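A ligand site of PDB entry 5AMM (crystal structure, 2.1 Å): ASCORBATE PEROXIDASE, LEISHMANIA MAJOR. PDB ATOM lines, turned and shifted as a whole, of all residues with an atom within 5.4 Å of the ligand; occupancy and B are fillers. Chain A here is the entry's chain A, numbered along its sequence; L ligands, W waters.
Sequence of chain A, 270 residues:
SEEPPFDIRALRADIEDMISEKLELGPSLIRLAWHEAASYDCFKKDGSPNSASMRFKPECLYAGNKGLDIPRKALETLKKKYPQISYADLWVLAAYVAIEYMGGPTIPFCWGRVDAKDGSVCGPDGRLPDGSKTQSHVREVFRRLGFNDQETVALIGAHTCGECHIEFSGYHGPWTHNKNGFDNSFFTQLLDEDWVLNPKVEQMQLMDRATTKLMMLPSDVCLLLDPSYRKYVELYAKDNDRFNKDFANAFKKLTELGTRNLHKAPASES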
ATOM      1  N   GLU A  24      21.153 -18.949  14.922  1.00  0.00           N
ATOM      2  CA  GLU A  24      20.130 -19.570  15.779  1.00  0.00           C
ATOM      3  C   GLU A  24      20.095 -18.995  17.190  1.00  0.00           C
ATOM      4  O   GLU A  24      19.142 -19.197  17.892  1.00  0.00           O
ATOM      5  CB  GLU A  24      20.227 -21.120  15.807  1.00  0.00           C
ATOM      6  CG  GLU A  24      21.540 -21.722  16.264  1.00  0.00           C
ATOM      7  CD  GLU A  24      22.668 -21.686  15.216  1.00  0.00           C
ATOM      8  OE1 GLU A  24      22.445 -21.348  14.016  1.00  0.00           O
ATOM      9  OE2 GLU A  24      23.797 -22.011  15.621  1.00  0.00           O
ATOM     10  N   PRO A  27      16.709 -16.165  17.749  1.00  0.00           N
ATOM     11  CA  PRO A  27      15.452 -16.581  18.413  1.00  0.00           C
ATOM     12  C   PRO A  27      15.614 -16.990  19.905  1.00  0.00           C
ATOM     13  O   PRO A  27      14.710 -16.738  20.700  1.00  0.00           O
ATOM     14  CB  PRO A  27      14.961 -17.738  17.547  1.00  0.00           C
ATOM     15  CG  PRO A  27      15.611 -17.477  16.187  1.00  0.00           C
ATOM     16  CD  PRO A  27      16.955 -16.885  16.493  1.00  0.00           C
ATOM     17  N   SER A  28      16.728 -17.615  20.291  1.00  0.00           N
ATOM     18  CA  SER A  28      16.815 -18.012  21.730  1.00  0.00           C
ATOM     19  C   SER A  28      16.956 -16.827  22.674  1.00  0.00           C
ATOM     20  O   SER A  28      16.514 -16.921  23.816  1.00  0.00           O
ATOM     21  CB  SER A  28      17.869 -19.102  22.004  1.00  0.00           C
ATOM     22  OG  SER A  28      19.113 -18.628  21.677  1.00  0.00           O
ATOM     23  N   ILE A  30      15.338 -14.015  22.294  1.00  0.00           N
ATOM     24  CA  ILE A  30      13.971 -13.494  22.426  1.00  0.00           C
ATOM     25  C   ILE A  30      13.262 -14.354  23.455  1.00  0.00           C
ATOM     26  O   ILE A  30      12.535 -13.835  24.364  1.00  0.00           O
ATOM     27  CB  ILE A  30      13.226 -13.527  21.058  1.00  0.00           C
ATOM     28  CG1 ILE A  30      13.882 -12.569  20.075  1.00  0.00           C
ATOM     29  CG2 ILE A  30      11.774 -13.206  21.233  1.00  0.00           C
ATOM     30  CD1 ILE A  30      13.295 -12.610  18.679  1.00  0.00           C
ATOM     31  N   ARG A  31      13.462 -15.675  23.337  1.00  0.00           N
ATOM     32  CA  ARG A  31      12.787 -16.606  24.261  1.00  0.00           C
ATOM     33  C   ARG A  31      13.319 -16.435  25.645  1.00  0.00           C
ATOM     34  O   ARG A  31      12.566 -16.548  26.613  1.00  0.00           O
ATOM     35  CB  ARG A  31      12.999 -18.044  23.838  1.00  0.00           C
ATOM     36  CG  ARG A  31      12.370 -19.100  24.730  1.00  0.00           C
ATOM     37  CD  ARG A  31      12.848 -20.471  24.328  1.00  0.00           C
ATOM     38  NE  ARG A  31      12.350 -21.503  25.219  1.00  0.00           N
ATOM     39  CZ  ARG A  31      13.032 -22.563  25.615  1.00  0.00           C
ATOM     40  NH1 ARG A  31      14.277 -22.799  25.207  1.00  0.00           N
ATOM     41  NH2 ARG A  31      12.454 -23.397  26.445  1.00  0.00           N
ATOM     42  N   TRP A  34      11.656 -13.287  27.124  1.00  0.00           N
ATOM     43  CA  TRP A  34      10.233 -13.616  27.348  1.00  0.00           C
ATOM     44  C   TRP A  34      10.076 -14.489  28.593  1.00  0.00           C
ATOM     45  O   TRP A  34       9.300 -14.158  29.489  1.00  0.00           O
ATOM     46  CB  TRP A  34       9.604 -14.240  26.070  1.00  0.00           C
ATOM     47  CG  TRP A  34       8.668 -15.375  26.182  1.00  0.00           C
ATOM     48  CD1 TRP A  34       8.804 -16.602  25.590  1.00  0.00           C
ATOM     49  CD2 TRP A  34       7.370 -15.378  26.797  1.00  0.00           C
ATOM     50  NE1 TRP A  34       7.697 -17.399  25.844  1.00  0.00           N
ATOM     51  CE2 TRP A  34       6.801 -16.666  26.586  1.00  0.00           C
ATOM     52  CE3 TRP A  34       6.648 -14.450  27.525  1.00  0.00           C
ATOM     53  CZ2 TRP A  34       5.571 -17.043  27.113  1.00  0.00           C
ATOM     54  CZ3 TRP A  34       5.391 -14.812  28.012  1.00  0.00           C
ATOM     55  CH2 TRP A  34       4.856 -16.095  27.799  1.00  0.00           C
ATOM     56  N   LYS A  66      14.243 -25.075  29.824  1.00  0.00           N
ATOM     57  CA  LYS A  66      15.304 -25.932  29.387  1.00  0.00           C
ATOM     58  C   LYS A  66      15.934 -25.437  28.079  1.00  0.00           C
ATOM     59  O   LYS A  66      15.260 -24.986  27.148  1.00  0.00           O
ATOM     60  CB  LYS A  66      14.803 -27.361  29.295  1.00  0.00           C
ATOM     61  CG  LYS A  66      15.964 -28.303  29.064  1.00  0.00           C
ATOM     62  CD  LYS A  66      15.529 -29.740  29.178  1.00  0.00           C
ATOM     63  CE  LYS A  66      16.777 -30.600  29.268  1.00  0.00           C
ATOM     64  NZ  LYS A  66      16.388 -32.012  29.030  1.00  0.00           N
ATOM     65  N   PRO A 129       3.829 -21.030  30.112  1.00  0.00           N
ATOM     66  CA  PRO A 129       2.720 -21.699  29.435  1.00  0.00           C
ATOM     67  C   PRO A 129       3.112 -23.037  28.834  1.00  0.00           C
ATOM     68  O   PRO A 129       4.246 -23.212  28.477  1.00  0.00           O
ATOM     69  CB  PRO A 129       2.314 -20.710  28.356  1.00  0.00           C
ATOM     70  CG  PRO A 129       3.546 -19.936  28.085  1.00  0.00           C
ATOM     71  CD  PRO A 129       4.358 -19.891  29.330  1.00  0.00           C
ATOM     72  N   ASP A 130       2.147 -23.937  28.740  1.00  0.00           N
ATOM     73  CA  ASP A 130       2.288 -25.326  28.319  1.00  0.00           C
ATOM     74  C   ASP A 130       1.783 -25.478  26.849  1.00  0.00           C
ATOM     75  O   ASP A 130       0.598 -25.323  26.559  1.00  0.00           O
ATOM     76  CB  ASP A 130       1.447 -26.181  29.290  1.00  0.00           C
ATOM     77  CG  ASP A 130       1.623 -27.685  29.099  1.00  0.00           C
ATOM     78  OD1 ASP A 130       1.987 -28.152  28.005  1.00  0.00           O
ATOM     79  OD2 ASP A 130       1.347 -28.421  30.043  1.00  0.00           O
ATOM     80  N   GLY A 131       2.686 -25.768  25.918  1.00  0.00           N
ATOM     81  CA  GLY A 131       2.369 -25.940  24.509  1.00  0.00           C
ATOM     82  C   GLY A 131       1.374 -27.038  24.200  1.00  0.00           C
ATOM     83  O   GLY A 131       0.789 -27.014  23.115  1.00  0.00           O
ATOM     84  N   VAL A 138      -4.148 -20.767  27.742  1.00  0.00           N
ATOM     85  CA  VAL A 138      -3.435 -19.637  27.173  1.00  0.00           C
ATOM     86  C   VAL A 138      -3.979 -18.307  27.757  1.00  0.00           C
ATOM     87  O   VAL A 138      -3.193 -17.444  28.209  1.00  0.00           O
ATOM     88  CB  VAL A 138      -3.477 -19.664  25.632  1.00  0.00           C
ATOM     89  CG1 VAL A 138      -2.883 -18.375  25.042  1.00  0.00           C
ATOM     90  CG2 VAL A 138      -2.734 -20.865  25.083  1.00  0.00           C
ATOM     91  N   PHE A 142      -1.925 -15.513  30.051  1.00  0.00           N
ATOM     92  CA  PHE A 142      -1.777 -14.139  29.642  1.00  0.00           C
ATOM     93  C   PHE A 142      -2.629 -13.132  30.453  1.00  0.00           C
ATOM     94  O   PHE A 142      -2.169 -12.003  30.681  1.00  0.00           O
ATOM     95  CB  PHE A 142      -1.973 -14.068  28.127  1.00  0.00           C
ATOM     96  CG  PHE A 142      -0.759 -14.543  27.353  1.00  0.00           C
ATOM     97  CD1 PHE A 142      -0.543 -15.888  27.139  1.00  0.00           C
ATOM     98  CD2 PHE A 142       0.184 -13.627  26.899  1.00  0.00           C
ATOM     99  CE1 PHE A 142       0.594 -16.343  26.419  1.00  0.00           C
ATOM    100  CE2 PHE A 142       1.326 -14.069  26.191  1.00  0.00           C
ATOM    101  CZ  PHE A 142       1.518 -15.423  25.943  1.00  0.00           C
ATOM    102  N   LEU A 155       2.050 -11.298  20.691  1.00  0.00           N
ATOM    103  CA  LEU A 155       3.259 -11.822  21.274  1.00  0.00           C
ATOM    104  C   LEU A 155       3.595 -13.213  20.792  1.00  0.00           C
ATOM    105  O   LEU A 155       4.766 -13.519  20.529  1.00  0.00           O
ATOM    106  CB  LEU A 155       3.160 -11.885  22.777  1.00  0.00           C
ATOM    107  CG  LEU A 155       3.259 -10.535  23.411  1.00  0.00           C
ATOM    108  CD1 LEU A 155       2.758 -10.628  24.855  1.00  0.00           C
ATOM    109  CD2 LEU A 155       4.695 -10.099  23.378  1.00  0.00           C
ATOM    110  N   ILE A 156       2.578 -14.075  20.696  1.00  0.00           N
ATOM    111  CA  ILE A 156       2.864 -15.431  20.248  1.00  0.00           C
ATOM    112  C   ILE A 156       3.332 -15.508  18.794  1.00  0.00           C
ATOM    113  O   ILE A 156       3.955 -16.485  18.368  1.00  0.00           O
ATOM    114  CB  ILE A 156       1.674 -16.339  20.491  1.00  0.00           C
ATOM    115  CG1 ILE A 156       1.407 -16.458  21.982  1.00  0.00           C
ATOM    116  CG2 ILE A 156       1.899 -17.701  19.870  1.00  0.00           C
ATOM    117  CD1 ILE A 156       0.031 -17.048  22.351  1.00  0.00           C
ATOM    118  N   ALA A 158       5.810 -14.232  17.695  1.00  0.00           N
ATOM    119  CA  ALA A 158       7.264 -14.377  17.692  1.00  0.00           C
ATOM    120  C   ALA A 158       7.748 -15.744  17.193  1.00  0.00           C
ATOM    121  O   ALA A 158       8.914 -15.901  16.838  1.00  0.00           O
ATOM    122  CB  ALA A 158       7.800 -14.145  19.095  1.00  0.00           C
ATOM    123  N   HIS A 159       6.856 -16.740  17.221  1.00  0.00           N
ATOM    124  CA  HIS A 159       7.133 -18.030  16.659  1.00  0.00           C
ATOM    125  C   HIS A 159       7.385 -17.980  15.144  1.00  0.00           C
ATOM    126  O   HIS A 159       7.756 -18.978  14.558  1.00  0.00           O
ATOM    127  CB  HIS A 159       6.015 -19.038  17.009  1.00  0.00           C
ATOM    128  CG  HIS A 159       5.992 -19.432  18.464  1.00  0.00           C
ATOM    129  ND1 HIS A 159       4.977 -20.174  19.032  1.00  0.00           N
ATOM    130  CD2 HIS A 159       6.893 -19.218  19.448  1.00  0.00           C
ATOM    131  CE1 HIS A 159       5.248 -20.378  20.304  1.00  0.00           C
ATOM    132  NE2 HIS A 159       6.400 -19.798  20.587  1.00  0.00           N
ATOM    133  N   CYS A 161       9.918 -16.813  14.206  1.00  0.00           N
ATOM    134  CA  CYS A 161      11.343 -17.150  14.132  1.00  0.00           C
ATOM    135  C   CYS A 161      11.747 -18.291  15.084  1.00  0.00           C
ATOM    136  O   CYS A 161      11.063 -18.551  16.063  1.00  0.00           O
ATOM    137  CB  CYS A 161      12.162 -15.886  14.339  1.00  0.00           C
ATOM    138  SG  CYS A 161      12.136 -15.308  16.021  1.00  0.00           S
ATOM    139  N   GLY A 162      12.844 -18.991  14.772  1.00  0.00           N
ATOM    140  CA  GLY A 162      13.338 -20.062  15.644  1.00  0.00           C
ATOM    141  C   GLY A 162      12.619 -21.376  15.398  1.00  0.00           C
ATOM    142  O   GLY A 162      11.831 -21.522  14.408  1.00  0.00           O
ATOM    143  N   GLU A 163      12.875 -22.330  16.293  1.00  0.00           N
ATOM    144  CA  GLU A 163      12.318 -23.637  16.160  1.00  0.00           C
ATOM    145  C   GLU A 163      12.255 -24.420  17.444  1.00  0.00           C
ATOM    146  O   GLU A 163      12.934 -24.093  18.422  1.00  0.00           O
ATOM    147  CB  GLU A 163      13.158 -24.412  15.130  1.00  0.00           C
ATOM    148  CG  GLU A 163      14.591 -24.615  15.533  1.00  0.00           C
ATOM    149  CD  GLU A 163      15.523 -25.001  14.363  1.00  0.00           C
ATOM    150  OE1 GLU A 163      15.089 -25.615  13.345  1.00  0.00           O
ATOM    151  OE2 GLU A 163      16.707 -24.627  14.469  1.00  0.00           O
ATOM    152  N   CYS A 164      11.475 -25.504  17.444  1.00  0.00           N
ATOM    153  CA  CYS A 164      11.427 -26.399  18.605  1.00  0.00           C
ATOM    154  C   CYS A 164      12.536 -27.446  18.521  1.00  0.00           C
ATOM    155  O   CYS A 164      12.844 -27.957  17.456  1.00  0.00           O
ATOM    156  CB  CYS A 164      10.049 -27.043  18.703  1.00  0.00           C
ATOM    157  SG  CYS A 164       8.730 -25.862  19.039  1.00  0.00           S
ATOM    158  N   HIS A 165      13.134 -27.776  19.655  1.00  0.00           N
ATOM    159  CA  HIS A 165      14.220 -28.773  19.704  1.00  0.00           C
ATOM    160  C   HIS A 165      13.794 -29.891  20.626  1.00  0.00           C
ATOM    161  O   HIS A 165      13.315 -29.648  21.784  1.00  0.00           O
ATOM    162  CB  HIS A 165      15.465 -28.131  20.248  1.00  0.00           C
ATOM    163  CG  HIS A 165      15.814 -26.820  19.619  1.00  0.00           C
ATOM    164  ND1 HIS A 165      15.317 -25.617  20.090  1.00  0.00           N
ATOM    165  CD2 HIS A 165      16.652 -26.508  18.609  1.00  0.00           C
ATOM    166  CE1 HIS A 165      15.843 -24.616  19.384  1.00  0.00           C
ATOM    167  NE2 HIS A 165      16.633 -25.137  18.460  1.00  0.00           N
ATOM    168  N   ILE A 166      13.908 -31.124  20.132  1.00  0.00           N
ATOM    169  CA  ILE A 166      13.463 -32.290  20.890  1.00  0.00           C
ATOM    170  C   ILE A 166      14.106 -32.314  22.283  1.00  0.00           C
ATOM    171  O   ILE A 166      13.448 -32.498  23.291  1.00  0.00           O
ATOM    172  CB  ILE A 166      13.837 -33.601  20.150  1.00  0.00           C
ATOM    173  CG1 ILE A 166      12.995 -33.759  18.900  1.00  0.00           C
ATOM    174  CG2 ILE A 166      13.693 -34.810  21.056  1.00  0.00           C
ATOM    175  CD1 ILE A 166      11.549 -34.075  19.171  1.00  0.00           C
ATOM    176  N   PHE A 168      14.968 -29.981  24.107  1.00  0.00           N
ATOM    177  CA  PHE A 168      14.595 -28.915  25.048  1.00  0.00           C
ATOM    178  C   PHE A 168      13.160 -28.966  25.495  1.00  0.00           C
ATOM    179  O   PHE A 168      12.882 -29.005  26.677  1.00  0.00           O
ATOM    180  CB  PHE A 168      14.915 -27.497  24.499  1.00  0.00           C
ATOM    181  CG  PHE A 168      16.374 -27.244  24.194  1.00  0.00           C
ATOM    182  CD1 PHE A 168      17.404 -28.012  24.775  1.00  0.00           C
ATOM    183  CD2 PHE A 168      16.725 -26.168  23.396  1.00  0.00           C
ATOM    184  CE1 PHE A 168      18.727 -27.744  24.482  1.00  0.00           C
ATOM    185  CE2 PHE A 168      18.044 -25.909  23.105  1.00  0.00           C
ATOM    186  CZ  PHE A 168      19.032 -26.689  23.653  1.00  0.00           C
ATOM    187  N   SER A 169      12.238 -28.936  24.553  1.00  0.00           N
ATOM    188  CA  SER A 169      10.826 -28.964  24.839  1.00  0.00           C
ATOM    189  C   SER A 169      10.205 -30.308  24.504  1.00  0.00           C
ATOM    190  O   SER A 169       9.039 -30.499  24.781  1.00  0.00           O
ATOM    191  CB  SER A 169      10.132 -27.939  23.931  1.00  0.00           C
ATOM    192  OG  SER A 169      10.441 -28.256  22.576  1.00  0.00           O
ATOM    193  N   GLY A 170      10.920 -31.182  23.791  1.00  0.00           N
ATOM    194  CA  GLY A 170      10.317 -32.405  23.261  1.00  0.00           C
ATOM    195  C   GLY A 170       9.478 -32.198  21.997  1.00  0.00           C
ATOM    196  O   GLY A 170       8.856 -33.124  21.501  1.00  0.00           O
ATOM    197  N   TYR A 171       9.398 -30.978  21.495  1.00  0.00           N
ATOM    198  CA  TYR A 171       8.733 -30.720  20.236  1.00  0.00           C
ATOM    199  C   TYR A 171       9.825 -30.574  19.143  1.00  0.00           C
ATOM    200  O   TYR A 171      11.042 -30.543  19.447  1.00  0.00           O
ATOM    201  CB  TYR A 171       7.878 -29.483  20.343  1.00  0.00           C
ATOM    202  CG  TYR A 171       6.651 -29.617  21.236  1.00  0.00           C
ATOM    203  CD1 TYR A 171       5.568 -30.421  20.861  1.00  0.00           C
ATOM    204  CD2 TYR A 171       6.570 -28.923  22.454  1.00  0.00           C
ATOM    205  CE1 TYR A 171       4.457 -30.546  21.669  1.00  0.00           C
ATOM    206  CE2 TYR A 171       5.466 -29.050  23.269  1.00  0.00           C
ATOM    207  CZ  TYR A 171       4.400 -29.827  22.856  1.00  0.00           C
ATOM    208  OH  TYR A 171       3.300 -29.945  23.670  1.00  0.00           O
ATOM    209  N   TRP A 175       8.261 -23.159  12.746  1.00  0.00           N
ATOM    210  CA  TRP A 175       6.894 -22.769  12.422  1.00  0.00           C
ATOM    211  C   TRP A 175       6.747 -22.244  11.000  1.00  0.00           C
ATOM    212  O   TRP A 175       5.677 -22.354  10.400  1.00  0.00           O
ATOM    213  CB  TRP A 175       6.375 -21.713  13.354  1.00  0.00           C
ATOM    214  CG  TRP A 175       6.181 -22.193  14.768  1.00  0.00           C
ATOM    215  CD1 TRP A 175       5.038 -22.708  15.334  1.00  0.00           C
ATOM    216  CD2 TRP A 175       7.165 -22.175  15.784  1.00  0.00           C
ATOM    217  NE1 TRP A 175       5.267 -22.999  16.667  1.00  0.00           N
ATOM    218  CE2 TRP A 175       6.574 -22.672  16.953  1.00  0.00           C
ATOM    219  CE3 TRP A 175       8.491 -21.716  15.834  1.00  0.00           C
ATOM    220  CZ2 TRP A 175       7.248 -22.748  18.139  1.00  0.00           C
ATOM    221  CZ3 TRP A 175       9.156 -21.821  16.984  1.00  0.00           C
ATOM    222  CH2 TRP A 175       8.547 -22.360  18.136  1.00  0.00           C
ATOM    223  N   LEU A 217       2.162 -26.084  17.459  1.00  0.00           N
ATOM    224  CA  LEU A 217       1.781 -26.658  18.741  1.00  0.00           C
ATOM    225  C   LEU A 217       0.268 -26.595  18.916  1.00  0.00           C
ATOM    226  O   LEU A 217      -0.343 -25.716  18.378  1.00  0.00           O
ATOM    227  CB  LEU A 217       2.371 -25.815  19.900  1.00  0.00           C
ATOM    228  CG  LEU A 217       3.870 -25.730  19.971  1.00  0.00           C
ATOM    229  CD1 LEU A 217       4.373 -24.546  20.792  1.00  0.00           C
ATOM    230  CD2 LEU A 217       4.411 -27.059  20.474  1.00  0.00           C
ATOM    231  N   SER A 219      -1.003 -25.153  21.417  1.00  0.00           N
ATOM    232  CA  SER A 219      -1.184 -23.793  21.869  1.00  0.00           C
ATOM    233  C   SER A 219      -1.220 -22.803  20.726  1.00  0.00           C
ATOM    234  O   SER A 219      -1.922 -21.777  20.817  1.00  0.00           O
ATOM    235  CB  SER A 219      -0.100 -23.385  22.885  1.00  0.00           C
ATOM    236  OG  SER A 219       1.197 -23.597  22.329  1.00  0.00           O
ATOM    237  N   PHE A 247       3.367  -5.840  18.050  1.00  0.00           N
ATOM    238  CA  PHE A 247       4.360  -6.706  18.674  1.00  0.00           C
ATOM    239  C   PHE A 247       5.337  -5.823  19.455  1.00  0.00           C
ATOM    240  O   PHE A 247       5.653  -6.094  20.613  1.00  0.00           O
ATOM    241  CB  PHE A 247       5.110  -7.611  17.675  1.00  0.00           C
ATOM    242  CG  PHE A 247       6.149  -8.476  18.379  1.00  0.00           C
ATOM    243  CD1 PHE A 247       5.798  -9.705  18.889  1.00  0.00           C
ATOM    244  CD2 PHE A 247       7.425  -8.016  18.591  1.00  0.00           C
ATOM    245  CE1 PHE A 247       6.679 -10.489  19.594  1.00  0.00           C
ATOM    246  CE2 PHE A 247       8.351  -8.787  19.299  1.00  0.00           C
ATOM    247  CZ  PHE A 247       7.974 -10.043  19.788  1.00  0.00           C
ATOM    248  N   PHE A 251       5.757  -6.322  23.517  1.00  0.00           N
ATOM    249  CA  PHE A 251       6.985  -6.917  23.929  1.00  0.00           C
ATOM    250  C   PHE A 251       7.688  -5.925  24.802  1.00  0.00           C
ATOM    251  O   PHE A 251       8.337  -6.299  25.792  1.00  0.00           O
ATOM    252  CB  PHE A 251       7.870  -7.305  22.747  1.00  0.00           C
ATOM    253  CG  PHE A 251       9.014  -8.213  23.131  1.00  0.00           C
ATOM    254  CD1 PHE A 251       8.811  -9.570  23.337  1.00  0.00           C
ATOM    255  CD2 PHE A 251      10.294  -7.738  23.236  1.00  0.00           C
ATOM    256  CE1 PHE A 251       9.836 -10.378  23.731  1.00  0.00           C
ATOM    257  CE2 PHE A 251      11.343  -8.570  23.592  1.00  0.00           C
ATOM    258  CZ  PHE A 251      11.112  -9.876  23.843  1.00  0.00           C
ATOM    259  N   LEU A 254       5.872  -6.301  27.996  1.00  0.00           N
ATOM    260  CA  LEU A 254       6.302  -7.566  28.564  1.00  0.00           C
ATOM    261  C   LEU A 254       7.626  -7.410  29.337  1.00  0.00           C
ATOM    262  O   LEU A 254       7.761  -7.851  30.465  1.00  0.00           O
ATOM    263  CB  LEU A 254       6.535  -8.572  27.461  1.00  0.00           C
ATOM    264  CG  LEU A 254       6.959  -9.957  27.923  1.00  0.00           C
ATOM    265  CD1 LEU A 254       5.811 -10.663  28.622  1.00  0.00           C
ATOM    266  CD2 LEU A 254       7.517 -10.805  26.778  1.00  0.00           C
HETATM  267  C1  LIG L   1      10.162 -21.454  21.272  1.00  0.00           C
HETATM  268  C2  LIG L   1       6.008 -22.661  23.530  1.00  0.00           C
HETATM  269  C3  LIG L   1       4.894 -17.977  23.742  1.00  0.00           C
HETATM  270  C4  LIG L   1       8.931 -16.891  21.579  1.00  0.00           C
HETATM  271  C5  LIG L   1       9.169 -22.154  21.946  1.00  0.00           C
HETATM  272  C6  LIG L   1       9.206 -23.532  22.184  1.00  0.00           C
HETATM  273  C7  LIG L   1       8.032 -23.877  22.761  1.00  0.00           C
HETATM  274  C8  LIG L   1       7.266 -22.704  22.928  1.00  0.00           C
HETATM  275  C9  LIG L   1       7.632 -25.284  23.167  1.00  0.00           C
HETATM  276  C10 LIG L   1      10.298 -24.508  21.794  1.00  0.00           C
HETATM  277  C11 LIG L   1      11.453 -24.496  22.809  1.00  0.00           C
HETATM  278  C12 LIG L   1      12.608 -25.404  22.363  1.00  0.00           C
HETATM  279  O1  LIG L   1      12.416 -26.625  22.171  1.00  0.00           O
HETATM  280  O2  LIG L   1      13.770 -24.963  22.141  1.00  0.00           O
HETATM  281  C13 LIG L   1       5.332 -21.447  23.759  1.00  0.00           C
HETATM  282  C14 LIG L   1       4.048 -21.347  24.352  1.00  0.00           C
HETATM  283  C15 LIG L   1       3.755 -20.042  24.454  1.00  0.00           C
HETATM  284  C16 LIG L   1       4.867 -19.348  23.810  1.00  0.00           C
HETATM  285  C17 LIG L   1       3.280 -22.522  24.869  1.00  0.00           C
HETATM  286  C18 LIG L   1       2.554 -19.299  24.808  1.00  0.00           C
HETATM  287  C19 LIG L   1       1.336 -19.811  24.566  1.00  0.00           C
HETATM  288  C20 LIG L   1       5.938 -17.230  23.283  1.00  0.00           C
HETATM  289  C21 LIG L   1       6.063 -15.829  23.374  1.00  0.00           C
HETATM  290  C22 LIG L   1       7.255 -15.527  22.801  1.00  0.00           C
HETATM  291  C23 LIG L   1       7.780 -16.749  22.276  1.00  0.00           C
HETATM  292  C24 LIG L   1       5.111 -14.878  24.010  1.00  0.00           C
HETATM  293  C25 LIG L   1       7.889 -14.215  22.564  1.00  0.00           C
HETATM  294  C26 LIG L   1       7.351 -13.034  22.764  1.00  0.00           C
HETATM  295  C27 LIG L   1       9.552 -18.090  21.266  1.00  0.00           C
HETATM  296  C28 LIG L   1      10.810 -18.110  20.496  1.00  0.00           C
HETATM  297  C29 LIG L   1      11.167 -19.403  20.434  1.00  0.00           C
HETATM  298  C30 LIG L   1      10.115 -20.117  21.156  1.00  0.00           C
HETATM  299  C31 LIG L   1      11.596 -16.930  19.912  1.00  0.00           C
HETATM  300  C32 LIG L   1      12.411 -19.947  19.716  1.00  0.00           C
HETATM  301  C33 LIG L   1      13.579 -20.436  20.591  1.00  0.00           C
HETATM  302  C34 LIG L   1      14.718 -20.988  19.737  1.00  0.00           C
HETATM  303  O3  LIG L   1      14.666 -21.077  18.485  1.00  0.00           O
HETATM  304  O4  LIG L   1      15.750 -21.394  20.291  1.00  0.00           O
HETATM  305  N1  LIG L   1       7.964 -21.664  22.385  1.00  0.00           N
HETATM  306  N2  LIG L   1       5.736 -20.226  23.441  1.00  0.00           N
HETATM  307  N3  LIG L   1       6.978 -17.758  22.622  1.00  0.00           N
HETATM  308  N4  LIG L   1       9.139 -19.303  21.634  1.00  0.00           N
HETATM  309 FE1  LIG L   1       7.497 -19.733  22.491  1.00  0.00          FE
HETATM  310  O   HOH W   1       1.755 -21.091  21.385  1.00  0.00           O
HETATM  311  O   HOH W   2       6.960 -20.406  26.337  1.00  0.00           O
HETATM  312  O   HOH W   3       8.750 -19.870  24.537  1.00  0.00           O
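A ring nitrogen (NE2) of His 159 is bound to an iron atom (FE1) of the ligand (2.2 Å). The backbone NH (N) of Ser 169 lies close to an oxygen (O1) of the ligand (3.3 Å). An oxygen (O1) of the ligand lies within hydrogen-bond range of the side-chain hydroxyl of Ser 169 (2.6 Å). O1 of the ligand lies within hydrogen-bond range of N of His 165 (2.9 Å). A ring nitrogen (ND1) of His 165 sits at hydrogen-bond distance from an oxygen (O2) of the ligand, at 2.7 Å. The backbone NH (N) of Glu 163 is in hydrogen-bond range of an oxygen (O3) of the ligand (3.1 Å). NH1 of Arg 31 is in salt-bridge range of O2 of the ligand.
The backbone carbonyl oxygen (O) of His 165 is in hydrogen-bond range of the side-chain hydroxyl (OG) of Ser 169, 3.3 Å away. OG of Ser 169 lies within hydrogen-bond range of N of Tyr 171 (3.1 Å). The backbone NH (N) of His 165 lies close to the backbone carbonyl oxygen (O) of Tyr 171 (3.5 Å). O of His 165 sits at hydrogen-bond distance from N of Gly 170, 3.5 Å away. The backbone NH (N) of Ser 219 is in hydrogen-bond range of the backbone carbonyl oxygen (O) of Gly 131 (3.1 Å). O of Ala 158 lies within hydrogen-bond range of SG of Cys 161, 3.4 Å away. NH1 of Arg 31 is in hydrogen-bond range of O of Lys 66 (3.1 Å). O of Tyr 171 lies within hydrogen-bond range of N of Ile 166.
The indole nitrogen of Trp 34 sits close to a nitrogen (N3) of the ligand, at 3.3 Å. Pro 27 touches the ligand (O to C31, 3.2 Å). CB of Ser 28 touches O4 of the ligand, at 3.6 Å. Ile 30 touches the ligand. Pro 129 touches the ligand. Asp 130 touches the ligand. N of Gly 131 touches C17 of the ligand, 3.5 Å away. CE1 of Phe 142 touches C18 of the ligand (3.9 Å). O of Leu 155 touches C26 of the ligand (3.5 Å). Ile 156 touches the ligand (CD1 to C19, 3.8 Å). CB of Ala 158 touches C25 of the ligand, at 3.5 Å. Gly 162 touches the ligand. SG of Cys 164 touches C10 of the ligand (3.4 Å). Phe 168 touches the ligand. Tyr 171 touches the ligand. CH2 of Trp 175 touches C1 of the ligand, 3.6 Å away. Leu 217 touches the ligand. OG of Ser 219 touches C17 of the ligand (3.5 Å). Phe 251 touches the ligand (CE1 to C26, 3.8 Å). Hydrophobic or aromatic side chains that line the ligand: Pro 27, Ile 30, Trp 34, Pro 129, Phe 142, Leu 155, Ile 156, Ala 158, His 159, His 165, Phe 168, Tyr 171, Trp 175, Leu 217 and Phe 251. 24 residues have an atom within 4 Å of the ligand: Pro 27, Ser 28, Ile 30, Arg 31, Trp 34, Pro 129, Asp 130, Gly 131, Phe 142, Leu 155, Ile 156, Ala 158, His 159, Gly 162, Glu 163, Cys 164, His 165, Phe 168, Ser 169, Tyr 171, Trp 175, Leu 217, Ser 219 and Phe 251.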
